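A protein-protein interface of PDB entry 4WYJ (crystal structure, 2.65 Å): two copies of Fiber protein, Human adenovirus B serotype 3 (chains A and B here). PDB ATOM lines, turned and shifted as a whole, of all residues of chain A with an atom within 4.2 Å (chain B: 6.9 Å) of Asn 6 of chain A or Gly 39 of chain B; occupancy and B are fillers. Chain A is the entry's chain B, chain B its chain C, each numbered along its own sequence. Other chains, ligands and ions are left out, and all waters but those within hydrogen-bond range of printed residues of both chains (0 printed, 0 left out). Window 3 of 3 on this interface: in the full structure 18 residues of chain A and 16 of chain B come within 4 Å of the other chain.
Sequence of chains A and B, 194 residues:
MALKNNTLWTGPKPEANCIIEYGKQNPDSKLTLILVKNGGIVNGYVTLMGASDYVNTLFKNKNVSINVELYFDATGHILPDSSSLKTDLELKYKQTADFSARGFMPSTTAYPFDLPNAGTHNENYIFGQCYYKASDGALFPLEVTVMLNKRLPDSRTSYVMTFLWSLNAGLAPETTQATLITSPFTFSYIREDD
The side-chain hydroxyl of Thr 7 of chain A is in hydrogen-bond range of the backbone NH of Gly 40 of chain B, at 3.1 Å.
The backbone carbonyl oxygen of Asn 6 of chain A is in hydrogen-bond range of the backbone NH of Lys 37 of chain A (2.8 Å).
The backbone carbonyl oxygen (O) of Gly 40 of chain B sits at hydrogen-bond distance from the backbone NH (N) of Arg 191 of chain B.
The backbone carbonyl oxygen (O) of Gly 39 of chain B lies within hydrogen-bond range of the guanidinium group (NE) of Arg 191 of chain B, at 2.8 Å.
The side-chain amide nitrogen (ND2) of Asn 6 of chain A lies close to the backbone NH (N) of Lys 4 of chain A, at 3.5 Å.
OD1 of Asn 6 of chain A touches CA of Gly 39 of chain B (3.7 Å).
CA of Gly 39 of chain B touches OG1 of Thr 7 of chain A, at 3.3 Å.
O of Asn 38 of chain B touches CG1 of Val 36 of chain A, at 3.4 Å.
Val 36 of chain A touches Gly 39 of chain B (CG1 to CA, 3.8 Å).
O of Lys 37 of chain A touches ND2 of Asn 38 of chain B (3.9 Å).
Asn 6 of chain A touches one residue of chain B.
Of chain A, only Asn 6 (3.7 Å), Thr 7 (3.3 Å) and Val 36 (3.8 Å) come within 4 Å of Gly 39 of chain B.
Printed residues of chain B within 4 Å of Val 36 of chain A: Asn 38 (3.4 Å) and Gly 39 (3.8 Å).
Of the printed residues of chain B, Thr 7 of chain A touches Gly 39 and Gly 40.
Printed residues of chain A within 4 Å of Asn 38 of chain B: Val 36 (3.4 Å) and Lys 37 (3.9 Å).
Leu 35 of chain A touches none of the printed residues of chain B.
Gly 103 of chain B touches none of the printed residues of chain A.
The nearest residue of chain B that does not touch Asn 6 of chain A is Gly 40 of chain B (5.3 Å).
The nearest printed residue of chain A that does not touch Gly 40 of chain B is Val 36 of chain A (4.4 Å).
Of the 10 printed residues of chain B, 3 touch a printed residue of chain A.
Of the 8 printed residues of chain A, 4 touch a printed residue of chain B.
Hydrophobic or aromatic side chains of chain A that line the printed part of chain B: Val 36.
Among the printed residues, no Asp or Glu carboxylate lies within 4 Å of a Lys or Arg side-chain nitrogen of the other chain.
Positions printed for both chains: 36 and 37.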
ATOM      1  N   LYS A   4     -13.322  -9.764  -2.977  1.00  0.00           N
ATOM      2  CA  LYS A   4     -14.678  -9.645  -3.515  1.00  0.00           C
ATOM      3  C   LYS A   4     -15.492 -10.925  -3.229  1.00  0.00           C
ATOM      4  O   LYS A   4     -15.242 -11.966  -3.852  1.00  0.00           O
ATOM      5  CB  LYS A   4     -14.656  -9.298  -5.022  1.00  0.00           C
ATOM      6  CG  LYS A   4     -14.066  -7.922  -5.329  1.00  0.00           C
ATOM      7  CD  LYS A   4     -14.011  -7.644  -6.825  1.00  0.00           C
ATOM      8  CE  LYS A   4     -13.578  -6.228  -7.129  1.00  0.00           C
ATOM      9  NZ  LYS A   4     -13.672  -5.927  -8.583  1.00  0.00           N
ATOM     10  N   ASN A   5     -16.452 -10.832  -2.261  1.00  0.00           N
ATOM     11  CA  ASN A   5     -17.360 -11.895  -1.776  1.00  0.00           C
ATOM     12  C   ASN A   5     -16.583 -13.056  -1.108  1.00  0.00           C
ATOM     13  O   ASN A   5     -17.053 -14.201  -1.146  1.00  0.00           O
ATOM     14  CB  ASN A   5     -18.278 -12.452  -2.906  1.00  0.00           C
ATOM     15  CG  ASN A   5     -18.837 -11.471  -3.924  1.00  0.00           C
ATOM     16  OD1 ASN A   5     -18.884 -10.249  -3.718  1.00  0.00           O
ATOM     17  ND2 ASN A   5     -19.309 -12.006  -5.049  1.00  0.00           N
ATOM     18  N   ASN A   6     -15.410 -12.774  -0.496  1.00  0.00           N
ATOM     19  CA  ASN A   6     -14.554 -13.845   0.051  1.00  0.00           C
ATOM     20  C   ASN A   6     -14.406 -13.912   1.593  1.00  0.00           C
ATOM     21  O   ASN A   6     -13.696 -14.787   2.066  1.00  0.00           O
ATOM     22  CB  ASN A   6     -13.162 -13.821  -0.599  1.00  0.00           C
ATOM     23  CG  ASN A   6     -12.444 -12.501  -0.551  1.00  0.00           C
ATOM     24  OD1 ASN A   6     -12.804 -11.573   0.196  1.00  0.00           O
ATOM     25  ND2 ASN A   6     -11.538 -12.325  -1.500  1.00  0.00           N
ATOM     26  N   THR A   7     -15.116 -13.070   2.361  1.00  0.00           N
ATOM     27  CA  THR A   7     -15.109 -13.086   3.832  1.00  0.00           C
ATOM     28  C   THR A   7     -16.527 -13.265   4.412  1.00  0.00           C
ATOM     29  O   THR A   7     -17.405 -12.431   4.194  1.00  0.00           O
ATOM     30  CB  THR A   7     -14.454 -11.823   4.406  1.00  0.00           C
ATOM     31  OG1 THR A   7     -13.207 -11.602   3.763  1.00  0.00           O
ATOM     32  CG2 THR A   7     -14.262 -11.894   5.897  1.00  0.00           C
ATOM     33  N   LEU A  35     -14.113 -16.418   8.272  1.00  0.00           N
ATOM     34  CA  LEU A  35     -13.868 -17.445   7.258  1.00  0.00           C
ATOM     35  C   LEU A  35     -13.554 -16.746   5.938  1.00  0.00           C
ATOM     36  O   LEU A  35     -14.410 -16.046   5.369  1.00  0.00           O
ATOM     37  CB  LEU A  35     -15.085 -18.403   7.120  1.00  0.00           C
ATOM     38  CG  LEU A  35     -15.513 -19.162   8.392  1.00  0.00           C
ATOM     39  CD1 LEU A  35     -16.844 -19.865   8.184  1.00  0.00           C
ATOM     40  CD2 LEU A  35     -14.407 -20.140   8.879  1.00  0.00           C
ATOM     41  N   VAL A  36     -12.303 -16.892   5.480  1.00  0.00           N
ATOM     42  CA  VAL A  36     -11.869 -16.245   4.237  1.00  0.00           C
ATOM     43  C   VAL A  36     -11.603 -17.295   3.147  1.00  0.00           C
ATOM     44  O   VAL A  36     -10.847 -18.230   3.383  1.00  0.00           O
ATOM     45  CB  VAL A  36     -10.662 -15.277   4.447  1.00  0.00           C
ATOM     46  CG1 VAL A  36     -10.329 -14.518   3.164  1.00  0.00           C
ATOM     47  CG2 VAL A  36     -10.912 -14.305   5.604  1.00  0.00           C
ATOM     48  N   LYS A  37     -12.234 -17.147   1.969  1.00  0.00           N
ATOM     49  CA  LYS A  37     -12.034 -18.014   0.804  1.00  0.00           C
ATOM     50  C   LYS A  37     -10.659 -17.659   0.217  1.00  0.00           C
ATOM     51  O   LYS A  37     -10.366 -16.470  -0.016  1.00  0.00           O
ATOM     52  CB  LYS A  37     -13.092 -17.736  -0.264  1.00  0.00           C
ATOM     53  CG  LYS A  37     -14.387 -18.492  -0.110  1.00  0.00           C
ATOM     54  CD  LYS A  37     -15.403 -17.953  -1.103  1.00  0.00           C
ATOM     55  CE  LYS A  37     -16.681 -18.743  -1.131  1.00  0.00           C
ATOM     56  NZ  LYS A  37     -17.718 -18.104  -2.001  1.00  0.00           N
ATOM     57  N   PHE A 104     -18.098 -21.507   1.577  1.00  0.00           N
ATOM     58  CA  PHE A 104     -17.334 -21.315   2.823  1.00  0.00           C
ATOM     59  C   PHE A 104     -17.411 -22.548   3.716  1.00  0.00           C
ATOM     60  O   PHE A 104     -16.762 -22.578   4.755  1.00  0.00           O
ATOM     61  CB  PHE A 104     -17.857 -20.098   3.611  1.00  0.00           C
ATOM     62  CG  PHE A 104     -17.576 -18.743   2.982  1.00  0.00           C
ATOM     63  CD1 PHE A 104     -18.471 -18.180   2.069  1.00  0.00           C
ATOM     64  CD2 PHE A 104     -16.433 -18.018   3.325  1.00  0.00           C
ATOM     65  CE1 PHE A 104     -18.228 -16.917   1.514  1.00  0.00           C
ATOM     66  CE2 PHE A 104     -16.174 -16.776   2.747  1.00  0.00           C
ATOM     67  CZ  PHE A 104     -17.070 -16.232   1.839  1.00  0.00           C
ATOM     68  N   VAL B  36       0.338 -10.018   3.944  1.00  0.00           N
ATOM     69  CA  VAL B  36      -0.499 -10.252   2.768  1.00  0.00           C
ATOM     70  C   VAL B  36      -1.984 -10.025   3.088  1.00  0.00           C
ATOM     71  O   VAL B  36      -2.492 -10.598   4.030  1.00  0.00           O
ATOM     72  CB  VAL B  36      -0.215 -11.635   2.107  1.00  0.00           C
ATOM     73  CG1 VAL B  36      -0.993 -11.796   0.812  1.00  0.00           C
ATOM     74  CG2 VAL B  36       1.276 -11.832   1.840  1.00  0.00           C
ATOM     75  N   LYS B  37      -2.662  -9.174   2.323  1.00  0.00           N
ATOM     76  CA  LYS B  37      -4.108  -8.907   2.429  1.00  0.00           C
ATOM     77  C   LYS B  37      -4.837 -10.137   1.887  1.00  0.00           C
ATOM     78  O   LYS B  37      -4.518 -10.616   0.789  1.00  0.00           O
ATOM     79  CB  LYS B  37      -4.512  -7.702   1.563  1.00  0.00           C
ATOM     80  CG  LYS B  37      -4.339  -6.354   2.213  1.00  0.00           C
ATOM     81  CD  LYS B  37      -4.555  -5.253   1.170  1.00  0.00           C
ATOM     82  CE  LYS B  37      -4.540  -3.897   1.786  1.00  0.00           C
ATOM     83  NZ  LYS B  37      -4.609  -2.836   0.752  1.00  0.00           N
ATOM     84  N   ASN B  38      -5.794 -10.662   2.655  1.00  0.00           N
ATOM     85  CA  ASN B  38      -6.580 -11.829   2.251  1.00  0.00           C
ATOM     86  C   ASN B  38      -7.951 -11.685   2.889  1.00  0.00           C
ATOM     87  O   ASN B  38      -8.146 -12.100   4.028  1.00  0.00           O
ATOM     88  CB  ASN B  38      -5.856 -13.134   2.669  1.00  0.00           C
ATOM     89  CG  ASN B  38      -6.556 -14.430   2.318  1.00  0.00           C
ATOM     90  OD1 ASN B  38      -6.456 -15.402   3.053  1.00  0.00           O
ATOM     91  ND2 ASN B  38      -7.265 -14.492   1.194  1.00  0.00           N
ATOM     92  N   GLY B  39      -8.858 -11.026   2.185  1.00  0.00           N
ATOM     93  CA  GLY B  39     -10.189 -10.728   2.697  1.00  0.00           C
ATOM     94  C   GLY B  39     -10.084  -9.731   3.837  1.00  0.00           C
ATOM     95  O   GLY B  39      -9.230  -8.844   3.793  1.00  0.00           O
ATOM     96  N   GLY B  40     -10.883  -9.918   4.886  1.00  0.00           N
ATOM     97  CA  GLY B  40     -10.851  -9.058   6.064  1.00  0.00           C
ATOM     98  C   GLY B  40      -9.655  -9.239   6.993  1.00  0.00           C
ATOM     99  O   GLY B  40      -9.547  -8.515   7.987  1.00  0.00           O
ATOM    100  N   ILE B  41      -8.758 -10.214   6.707  1.00  0.00           N
ATOM    101  CA  ILE B  41      -7.572 -10.475   7.528  1.00  0.00           C
ATOM    102  C   ILE B  41      -6.262 -10.213   6.763  1.00  0.00           C
ATOM    103  O   ILE B  41      -6.274 -10.124   5.531  1.00  0.00           O
ATOM    104  CB  ILE B  41      -7.584 -11.911   8.190  1.00  0.00           C
ATOM    105  CG1 ILE B  41      -7.354 -13.032   7.137  1.00  0.00           C
ATOM    106  CG2 ILE B  41      -8.843 -12.139   9.030  1.00  0.00           C
ATOM    107  CD1 ILE B  41      -7.293 -14.456   7.628  1.00  0.00           C
ATOM    108  N   VAL B  42      -5.140 -10.103   7.500  1.00  0.00           N
ATOM    109  CA  VAL B  42      -3.782 -10.002   6.957  1.00  0.00           C
ATOM    110  C   VAL B  42      -3.084 -11.290   7.368  1.00  0.00           C
ATOM    111  O   VAL B  42      -3.123 -11.638   8.557  1.00  0.00           O
ATOM    112  CB  VAL B  42      -2.967  -8.750   7.420  1.00  0.00           C
ATOM    113  CG1 VAL B  42      -1.456  -8.979   7.294  1.00  0.00           C
ATOM    114  CG2 VAL B  42      -3.374  -7.499   6.652  1.00  0.00           C
ATOM    115  N   GLY B 103      -4.650  -0.312   4.842  1.00  0.00           N
ATOM    116  CA  GLY B 103      -5.336  -1.594   4.709  1.00  0.00           C
ATOM    117  C   GLY B 103      -4.568  -2.798   5.233  1.00  0.00           C
ATOM    118  O   GLY B 103      -5.173  -3.851   5.438  1.00  0.00           O
ATOM    119  N   ARG B 191      -7.604  -6.817   9.763  1.00  0.00           N
ATOM    120  CA  ARG B 191      -7.008  -5.592   9.192  1.00  0.00           C
ATOM    121  C   ARG B 191      -7.936  -4.403   9.207  1.00  0.00           C
ATOM    122  O   ARG B 191      -9.157  -4.567   9.215  1.00  0.00           O
ATOM    123  CB  ARG B 191      -6.482  -5.815   7.770  1.00  0.00           C
ATOM    124  CG  ARG B 191      -7.553  -6.102   6.723  1.00  0.00           C
ATOM    125  CD  ARG B 191      -6.917  -6.547   5.416  1.00  0.00           C
ATOM    126  NE  ARG B 191      -7.846  -6.484   4.286  1.00  0.00           N
ATOM    127  CZ  ARG B 191      -8.086  -5.398   3.565  1.00  0.00           C
ATOM    128  NH1 ARG B 191      -7.472  -4.256   3.848  1.00  0.00           N
ATOM    129  NH2 ARG B 191      -8.957  -5.437   2.569  1.00  0.00           N
ATOM    130  N   ASP B 194      -9.112  -0.296   3.927  1.00  0.00           N
ATOM    131  CA  ASP B 194      -8.232   0.160   2.840  1.00  0.00           C
ATOM    132  C   ASP B 194      -8.053   1.688   2.767  1.00  0.00           C
ATOM    133  O   ASP B 194      -9.065   2.426   2.857  1.00  0.00           O
ATOM    134  CB  ASP B 194      -8.718  -0.382   1.485  1.00  0.00           C
ATOM    135  CG  ASP B 194      -8.547  -1.878   1.327  1.00  0.00           C
ATOM    136  OD1 ASP B 194      -7.409  -2.318   1.067  1.00  0.00           O
ATOM    137  OD2 ASP B 194      -9.560  -2.608   1.437  1.00  0.00           O
ATOM    138  OXT ASP B 194      -6.888   2.138   2.663  1.00  0.00           O
